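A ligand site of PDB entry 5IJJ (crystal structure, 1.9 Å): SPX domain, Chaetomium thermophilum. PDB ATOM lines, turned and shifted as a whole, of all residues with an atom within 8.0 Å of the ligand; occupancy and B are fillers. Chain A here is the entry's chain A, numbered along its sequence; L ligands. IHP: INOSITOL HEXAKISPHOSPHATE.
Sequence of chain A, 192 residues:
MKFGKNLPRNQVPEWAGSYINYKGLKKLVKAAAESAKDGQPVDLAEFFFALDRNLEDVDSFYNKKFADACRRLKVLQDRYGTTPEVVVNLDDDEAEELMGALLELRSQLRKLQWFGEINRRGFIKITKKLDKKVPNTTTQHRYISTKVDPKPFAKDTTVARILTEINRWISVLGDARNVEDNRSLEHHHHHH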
ATOM      1  N   MET A   1      -7.514   9.575 -13.771  1.00  0.00           N
ATOM      2  CA  MET A   1      -8.929   9.460 -13.316  1.00  0.00           C
ATOM      3  C   MET A   1      -8.961   8.995 -11.830  1.00  0.00           C
ATOM      4  O   MET A   1      -8.241   8.090 -11.461  1.00  0.00           O
ATOM      5  CB  MET A   1      -9.732   8.535 -14.250  1.00  0.00           C
ATOM      6  N   LYS A   2      -9.760   9.712 -11.005  1.00  0.00           N
ATOM      7  CA  LYS A   2     -10.169   9.387  -9.623  1.00  0.00           C
ATOM      8  C   LYS A   2     -10.923   8.067  -9.712  1.00  0.00           C
ATOM      9  O   LYS A   2     -12.009   8.008 -10.239  1.00  0.00           O
ATOM     10  CB  LYS A   2     -11.125  10.483  -9.088  1.00  0.00           C
ATOM     11  N   PHE A   3     -10.350   7.005  -9.197  1.00  0.00           N
ATOM     12  CA  PHE A   3     -10.991   5.703  -9.337  1.00  0.00           C
ATOM     13  C   PHE A   3     -12.028   5.454  -8.221  1.00  0.00           C
ATOM     14  O   PHE A   3     -13.158   5.067  -8.538  1.00  0.00           O
ATOM     15  CB  PHE A   3      -9.927   4.600  -9.303  1.00  0.00           C
ATOM     16  CG  PHE A   3     -10.492   3.266  -9.530  1.00  0.00           C
ATOM     17  CD1 PHE A   3     -10.809   2.468  -8.474  1.00  0.00           C
ATOM     18  CD2 PHE A   3     -10.881   2.889 -10.842  1.00  0.00           C
ATOM     19  CE1 PHE A   3     -11.385   1.227  -8.699  1.00  0.00           C
ATOM     20  CE2 PHE A   3     -11.433   1.682 -11.054  1.00  0.00           C
ATOM     21  CZ  PHE A   3     -11.688   0.840  -9.989  1.00  0.00           C
ATOM     22  N   GLY A   4     -11.594   5.624  -6.939  1.00  0.00           N
ATOM     23  CA  GLY A   4     -12.427   5.329  -5.734  1.00  0.00           C
ATOM     24  C   GLY A   4     -13.746   6.079  -5.690  1.00  0.00           C
ATOM     25  O   GLY A   4     -14.820   5.475  -5.474  1.00  0.00           O
ATOM     26  N   LYS A   5     -13.708   7.379  -5.940  1.00  0.00           N
ATOM     27  CA  LYS A   5     -14.939   8.163  -5.961  1.00  0.00           C
ATOM     28  C   LYS A   5     -15.901   7.765  -7.122  1.00  0.00           C
ATOM     29  O   LYS A   5     -17.125   7.865  -7.039  1.00  0.00           O
ATOM     30  CB  LYS A   5     -14.572   9.675  -6.022  1.00  0.00           C
ATOM     31  CG  LYS A   5     -15.752  10.612  -6.193  1.00  0.00           C
ATOM     32  CD  LYS A   5     -16.835  10.521  -5.111  1.00  0.00           C
ATOM     33  CE  LYS A   5     -18.215  10.966  -5.616  1.00  0.00           C
ATOM     34  NZ  LYS A   5     -18.987  11.635  -4.526  1.00  0.00           N
ATOM     35  N   ASN A   6     -15.344   7.306  -8.242  1.00  0.00           N
ATOM     36  CA  ASN A   6     -16.194   6.936  -9.390  1.00  0.00           C
ATOM     37  C   ASN A   6     -16.651   5.422  -9.346  1.00  0.00           C
ATOM     38  O   ASN A   6     -17.516   5.004 -10.154  1.00  0.00           O
ATOM     39  CB  ASN A   6     -15.438   7.231 -10.694  1.00  0.00           C
ATOM     40  CG  ASN A   6     -15.266   8.701 -10.959  1.00  0.00           C
ATOM     41  OD1 ASN A   6     -16.227   9.392 -11.105  1.00  0.00           O
ATOM     42  ND2 ASN A   6     -14.049   9.151 -11.136  1.00  0.00           N
ATOM     43  N   LEU A   7     -16.091   4.628  -8.420  1.00  0.00           N
ATOM     44  CA  LEU A   7     -16.356   3.176  -8.384  1.00  0.00           C
ATOM     45  C   LEU A   7     -17.831   2.784  -8.268  1.00  0.00           C
ATOM     46  O   LEU A   7     -18.322   2.080  -9.160  1.00  0.00           O
ATOM     47  CB  LEU A   7     -15.476   2.483  -7.313  1.00  0.00           C
ATOM     48  CG  LEU A   7     -15.539   0.963  -7.278  1.00  0.00           C
ATOM     49  CD1 LEU A   7     -15.359   0.428  -8.680  1.00  0.00           C
ATOM     50  CD2 LEU A   7     -14.521   0.341  -6.334  1.00  0.00           C
ATOM     51  N   TYR A  22     -11.643  -1.880  -3.499  1.00  0.00           N
ATOM     52  CA  TYR A  22     -10.645  -0.818  -3.597  1.00  0.00           C
ATOM     53  C   TYR A  22     -10.442  -0.110  -2.243  1.00  0.00           C
ATOM     54  O   TYR A  22      -9.334   0.212  -1.858  1.00  0.00           O
ATOM     55  CB  TYR A  22     -11.036   0.207  -4.641  1.00  0.00           C
ATOM     56  CG  TYR A  22      -9.940   1.135  -5.073  1.00  0.00           C
ATOM     57  CD1 TYR A  22      -9.004   0.754  -6.049  1.00  0.00           C
ATOM     58  CD2 TYR A  22      -9.909   2.443  -4.607  1.00  0.00           C
ATOM     59  CE1 TYR A  22      -8.046   1.634  -6.467  1.00  0.00           C
ATOM     60  CE2 TYR A  22      -8.918   3.328  -5.000  1.00  0.00           C
ATOM     61  CZ  TYR A  22      -7.997   2.915  -5.936  1.00  0.00           C
ATOM     62  OH  TYR A  22      -7.040   3.790  -6.363  1.00  0.00           O
ATOM     63  N   LYS A  23     -11.537   0.082  -1.565  1.00  0.00           N
ATOM     64  CA  LYS A  23     -11.618   0.752  -0.279  1.00  0.00           C
ATOM     65  C   LYS A  23     -10.753   0.014   0.759  1.00  0.00           C
ATOM     66  O   LYS A  23      -9.858   0.620   1.381  1.00  0.00           O
ATOM     67  CB  LYS A  23     -13.086   0.905   0.145  1.00  0.00           C
ATOM     68  CG  LYS A  23     -13.186   1.324   1.600  1.00  0.00           C
ATOM     69  CD  LYS A  23     -14.472   2.040   1.969  1.00  0.00           C
ATOM     70  CE  LYS A  23     -14.372   2.604   3.388  1.00  0.00           C
ATOM     71  NZ  LYS A  23     -15.757   2.940   3.889  1.00  0.00           N
ATOM     72  N   LYS A  26      -7.000   0.232  -0.099  1.00  0.00           N
ATOM     73  CA  LYS A  26      -6.443   1.495   0.220  1.00  0.00           C
ATOM     74  C   LYS A  26      -6.035   1.630   1.657  1.00  0.00           C
ATOM     75  O   LYS A  26      -5.028   2.245   1.897  1.00  0.00           O
ATOM     76  CB  LYS A  26      -7.400   2.617  -0.022  1.00  0.00           C
ATOM     77  CG  LYS A  26      -7.520   3.021  -1.431  1.00  0.00           C
ATOM     78  CD  LYS A  26      -8.434   4.303  -1.488  1.00  0.00           C
ATOM     79  CE  LYS A  26      -7.695   5.544  -1.043  1.00  0.00           C
ATOM     80  NZ  LYS A  26      -8.705   6.534  -0.595  1.00  0.00           N
ATOM     81  N   LYS A  27      -6.762   1.035   2.606  1.00  0.00           N
ATOM     82  CA  LYS A  27      -6.343   1.047   4.034  1.00  0.00           C
ATOM     83  C   LYS A  27      -5.069   0.256   4.264  1.00  0.00           C
ATOM     84  O   LYS A  27      -4.230   0.636   5.050  1.00  0.00           O
ATOM     85  CB  LYS A  27      -7.414   0.456   4.995  1.00  0.00           C
ATOM     86  CG  LYS A  27      -8.849   0.759   4.645  1.00  0.00           C
ATOM     87  CD  LYS A  27      -9.780   0.695   5.868  1.00  0.00           C
ATOM     88  CE  LYS A  27     -11.014   1.557   5.619  1.00  0.00           C
ATOM     89  NZ  LYS A  27     -12.186   0.887   6.210  1.00  0.00           N
ATOM     90  N   VAL A  29      -2.753   0.089   2.006  1.00  0.00           N
ATOM     91  CA  VAL A  29      -1.736   0.960   1.458  1.00  0.00           C
ATOM     92  C   VAL A  29      -1.393   2.012   2.476  1.00  0.00           C
ATOM     93  O   VAL A  29      -0.243   2.353   2.666  1.00  0.00           O
ATOM     94  CB  VAL A  29      -2.121   1.624   0.104  1.00  0.00           C
ATOM     95  CG1 VAL A  29      -1.046   2.640  -0.355  1.00  0.00           C
ATOM     96  CG2 VAL A  29      -2.338   0.557  -0.973  1.00  0.00           C
ATOM     97  N   LYS A  30      -2.428   2.628   3.042  1.00  0.00           N
ATOM     98  CA  LYS A  30      -2.202   3.664   3.987  1.00  0.00           C
ATOM     99  C   LYS A  30      -1.382   3.169   5.185  1.00  0.00           C
ATOM    100  O   LYS A  30      -0.482   3.874   5.624  1.00  0.00           O
ATOM    101  CB  LYS A  30      -3.533   4.319   4.404  1.00  0.00           C
ATOM    102  CG  LYS A  30      -4.076   5.154   3.253  1.00  0.00           C
ATOM    103  CD  LYS A  30      -5.350   5.950   3.548  1.00  0.00           C
ATOM    104  CE  LYS A  30      -6.021   6.416   2.271  1.00  0.00           C
ATOM    105  NZ  LYS A  30      -7.441   6.827   2.462  1.00  0.00           N
ATOM    106  N   ALA A  33       2.136   3.091   4.116  1.00  0.00           N
ATOM    107  CA  ALA A  33       2.613   4.457   3.939  1.00  0.00           C
ATOM    108  C   ALA A  33       2.955   5.058   5.298  1.00  0.00           C
ATOM    109  O   ALA A  33       3.965   5.785   5.393  1.00  0.00           O
ATOM    110  CB  ALA A  33       1.573   5.315   3.232  1.00  0.00           C
ATOM    111  N   GLY A 122      -9.024  -0.791 -11.702  1.00  0.00           N
ATOM    112  CA  GLY A 122      -8.813  -0.808 -10.293  1.00  0.00           C
ATOM    113  C   GLY A 122      -7.509  -1.440  -9.852  1.00  0.00           C
ATOM    114  O   GLY A 122      -6.821  -0.904  -8.981  1.00  0.00           O
ATOM    115  N   LYS A 125      -4.776   1.062 -10.782  1.00  0.00           N
ATOM    116  CA  LYS A 125      -4.747   2.247  -9.898  1.00  0.00           C
ATOM    117  C   LYS A 125      -4.238   1.976  -8.484  1.00  0.00           C
ATOM    118  O   LYS A 125      -3.496   2.761  -7.956  1.00  0.00           O
ATOM    119  CB  LYS A 125      -6.117   2.869  -9.873  1.00  0.00           C
ATOM    120  CG  LYS A 125      -6.386   3.644 -11.132  1.00  0.00           C
ATOM    121  CD  LYS A 125      -5.840   5.076 -11.117  1.00  0.00           C
ATOM    122  CE  LYS A 125      -6.006   5.806  -9.790  1.00  0.00           C
ATOM    123  NZ  LYS A 125      -5.855   7.329  -9.841  1.00  0.00           N
ATOM    124  N   ILE A 126      -4.589   0.801  -7.915  1.00  0.00           N
ATOM    125  CA  ILE A 126      -4.199   0.501  -6.535  1.00  0.00           C
ATOM    126  C   ILE A 126      -2.698   0.229  -6.391  1.00  0.00           C
ATOM    127  O   ILE A 126      -2.066   0.655  -5.413  1.00  0.00           O
ATOM    128  CB  ILE A 126      -5.109  -0.578  -5.927  1.00  0.00           C
ATOM    129  CG1 ILE A 126      -4.987  -0.614  -4.438  1.00  0.00           C
ATOM    130  CG2 ILE A 126      -4.728  -1.979  -6.464  1.00  0.00           C
ATOM    131  CD1 ILE A 126      -5.565   0.594  -3.663  1.00  0.00           C
ATOM    132  N   LYS A 128      -0.438   1.405  -8.612  1.00  0.00           N
ATOM    133  CA  LYS A 128       0.157   2.667  -8.804  1.00  0.00           C
ATOM    134  C   LYS A 128       0.173   3.479  -7.513  1.00  0.00           C
ATOM    135  O   LYS A 128       1.113   4.269  -7.223  1.00  0.00           O
ATOM    136  CB  LYS A 128      -0.625   3.415  -9.861  1.00  0.00           C
ATOM    137  CG  LYS A 128      -0.100   4.771 -10.222  1.00  0.00           C
ATOM    138  CD  LYS A 128      -1.073   5.479 -11.182  1.00  0.00           C
ATOM    139  CE  LYS A 128      -1.987   6.478 -10.406  1.00  0.00           C
ATOM    140  NZ  LYS A 128      -2.296   7.844 -10.977  1.00  0.00           N
ATOM    141  N   LYS A 129      -0.937   3.421  -6.802  1.00  0.00           N
ATOM    142  CA  LYS A 129      -1.034   4.119  -5.549  1.00  0.00           C
ATOM    143  C   LYS A 129       0.063   3.636  -4.505  1.00  0.00           C
ATOM    144  O   LYS A 129       0.781   4.455  -3.876  1.00  0.00           O
ATOM    145  CB  LYS A 129      -2.427   3.955  -4.929  1.00  0.00           C
ATOM    146  CG  LYS A 129      -2.546   4.663  -3.543  1.00  0.00           C
ATOM    147  CD  LYS A 129      -3.880   4.485  -2.825  1.00  0.00           C
ATOM    148  CE  LYS A 129      -5.061   4.932  -3.714  1.00  0.00           C
ATOM    149  NZ  LYS A 129      -5.093   6.433  -3.769  1.00  0.00           N
ATOM    150  N   LEU A 130       0.136   2.298  -4.322  1.00  0.00           N
ATOM    151  CA  LEU A 130       1.200   1.721  -3.474  1.00  0.00           C
ATOM    152  C   LEU A 130       2.599   2.221  -3.842  1.00  0.00           C
ATOM    153  O   LEU A 130       3.350   2.694  -2.951  1.00  0.00           O
ATOM    154  CB  LEU A 130       1.109   0.190  -3.519  1.00  0.00           C
ATOM    155  CG  LEU A 130       2.112  -0.528  -2.671  1.00  0.00           C
ATOM    156  CD1 LEU A 130       1.649  -0.572  -1.246  1.00  0.00           C
ATOM    157  CD2 LEU A 130       2.348  -1.973  -3.206  1.00  0.00           C
ATOM    158  N   LYS A 132       3.470   4.892  -5.332  1.00  0.00           N
ATOM    159  CA  LYS A 132       3.583   6.349  -5.154  1.00  0.00           C
ATOM    160  C   LYS A 132       3.751   6.613  -3.648  1.00  0.00           C
ATOM    161  O   LYS A 132       4.467   7.517  -3.296  1.00  0.00           O
ATOM    162  CB  LYS A 132       2.250   6.952  -5.755  1.00  0.00           C
ATOM    163  CG  LYS A 132       2.116   8.409  -6.052  1.00  0.00           C
ATOM    164  CD  LYS A 132       0.867   8.602  -6.897  1.00  0.00           C
ATOM    165  CE  LYS A 132       0.291   9.986  -6.735  1.00  0.00           C
ATOM    166  NZ  LYS A 132      -1.201   9.905  -6.800  1.00  0.00           N
ATOM    167  N   LYS A 133       3.150   5.796  -2.782  1.00  0.00           N
ATOM    168  CA  LYS A 133       3.078   6.074  -1.320  1.00  0.00           C
ATOM    169  C   LYS A 133       4.088   5.328  -0.460  1.00  0.00           C
ATOM    170  O   LYS A 133       4.205   5.613   0.719  1.00  0.00           O
ATOM    171  CB  LYS A 133       1.701   5.758  -0.730  1.00  0.00           C
ATOM    172  CG  LYS A 133       0.524   6.401  -1.367  1.00  0.00           C
ATOM    173  CD  LYS A 133       0.458   7.866  -1.117  1.00  0.00           C
ATOM    174  CE  LYS A 133      -0.868   8.331  -1.698  1.00  0.00           C
ATOM    175  NZ  LYS A 133      -0.962   9.779  -1.481  1.00  0.00           N
HETATM  176  C1  IHP L   1      -5.666  10.428  -3.639  1.00  0.00           C
HETATM  177  C2  IHP L   1      -6.579  10.349  -4.838  1.00  0.00           C
HETATM  178  C3  IHP L   1      -7.930   9.700  -4.654  1.00  0.00           C
HETATM  179  C4  IHP L   1      -8.626  10.113  -3.375  1.00  0.00           C
HETATM  180  C5  IHP L   1      -7.780   9.941  -2.123  1.00  0.00           C
HETATM  181  C6  IHP L   1      -6.309  10.219  -2.272  1.00  0.00           C
HETATM  182  O11 IHP L   1      -5.007  11.687  -3.650  1.00  0.00           O
HETATM  183  P1  IHP L   1      -3.496  11.900  -3.090  1.00  0.00           P
HETATM  184  O21 IHP L   1      -3.164  13.268  -3.614  1.00  0.00           O
HETATM  185  O31 IHP L   1      -3.612  11.904  -1.579  1.00  0.00           O
HETATM  186  O41 IHP L   1      -2.743  10.716  -3.705  1.00  0.00           O
HETATM  187  O12 IHP L   1      -5.825   9.560  -5.743  1.00  0.00           O
HETATM  188  P2  IHP L   1      -5.068  10.100  -7.064  1.00  0.00           P
HETATM  189  O22 IHP L   1      -3.711   9.429  -7.063  1.00  0.00           O
HETATM  190  O32 IHP L   1      -4.906  11.571  -6.834  1.00  0.00           O
HETATM  191  O42 IHP L   1      -6.068   9.573  -8.099  1.00  0.00           O
HETATM  192  O13 IHP L   1      -7.753   8.308  -4.632  1.00  0.00           O
HETATM  193  P3  IHP L   1      -8.350   7.215  -5.677  1.00  0.00           P
HETATM  194  O23 IHP L   1      -9.729   6.881  -5.202  1.00  0.00           O
HETATM  195  O33 IHP L   1      -8.282   7.796  -7.080  1.00  0.00           O
HETATM  196  O43 IHP L   1      -7.347   6.085  -5.506  1.00  0.00           O
HETATM  197  O14 IHP L   1      -9.691   9.208  -3.072  1.00  0.00           O
HETATM  198  P4  IHP L   1     -11.257   9.391  -3.308  1.00  0.00           P
HETATM  199  O24 IHP L   1     -11.824   8.364  -2.357  1.00  0.00           O
HETATM  200  O34 IHP L   1     -11.521  10.829  -2.877  1.00  0.00           O
HETATM  201  O44 IHP L   1     -11.504   9.072  -4.785  1.00  0.00           O
HETATM  202  O15 IHP L   1      -8.261  10.737  -1.042  1.00  0.00           O
HETATM  203  P5  IHP L   1      -8.601  10.195   0.444  1.00  0.00           P
HETATM  204  O25 IHP L   1      -8.215   8.727   0.500  1.00  0.00           O
HETATM  205  O35 IHP L   1     -10.102  10.402   0.567  1.00  0.00           O
HETATM  206  O45 IHP L   1      -7.690  11.135   1.195  1.00  0.00           O
HETATM  207  O16 IHP L   1      -5.857   8.929  -1.954  1.00  0.00           O
HETATM  208  P6  IHP L   1      -4.940   8.617  -0.702  1.00  0.00           P
HETATM  209  O26 IHP L   1      -3.759   9.499  -1.070  1.00  0.00           O
HETATM  210  O36 IHP L   1      -4.857   7.096  -0.894  1.00  0.00           O
HETATM  211  O46 IHP L   1      -5.690   9.137   0.489  1.00  0.00           O
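CA of Lys 2 touches O33 of the ligand (3.5 Å).
Hydrophobic or aromatic side chains within 4 Å of the ligand: Tyr 22.
Within 4 Å of the ligand: Lys 2, Phe 3, Gly 4, Lys 5, Tyr 22, Lys 26, Lys 30, Lys 125, Lys 129, Lys 132 and Lys 133.
The nearest printed residue that does not touch the ligand is Met 1 (4.3 Å).
O of Lys 2 sits at hydrogen-bond distance from ND2 of Asn 6 (2.5 Å).
O of Met 1 lies within hydrogen-bond range of NZ of Lys 125.
NZ of Lys 125 is in salt-bridge range of O42 of the ligand, at 2.8 Å.
O25 of the ligand is in salt-bridge range of NZ of Lys 26, 2.5 Å away.
The backbone NH (N) of Lys 5 is in hydrogen-bond range of an oxygen (O44) of the ligand (3.0 Å).
An oxygen (O23) of the ligand is in hydrogen-bond range of the backbone NH (N) of Gly 4.
O26 of the ligand is in salt-bridge range of NZ of Lys 133.
O43 of the ligand lies within salt-bridge range of NZ of Lys 129, 2.9 Å away.
NZ of Lys 30 lies within salt-bridge range of O25 of the ligand, at 2.8 Å.
The side-chain amino group of Lys 132 lies within salt-bridge range of an oxygen (O22) of the ligand.
An oxygen (O33) of the ligand sits at hydrogen-bond distance from the backbone NH of Phe 3, 3.1 Å away.
O43 of the ligand is in hydrogen-bond range of OH of Tyr 22.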
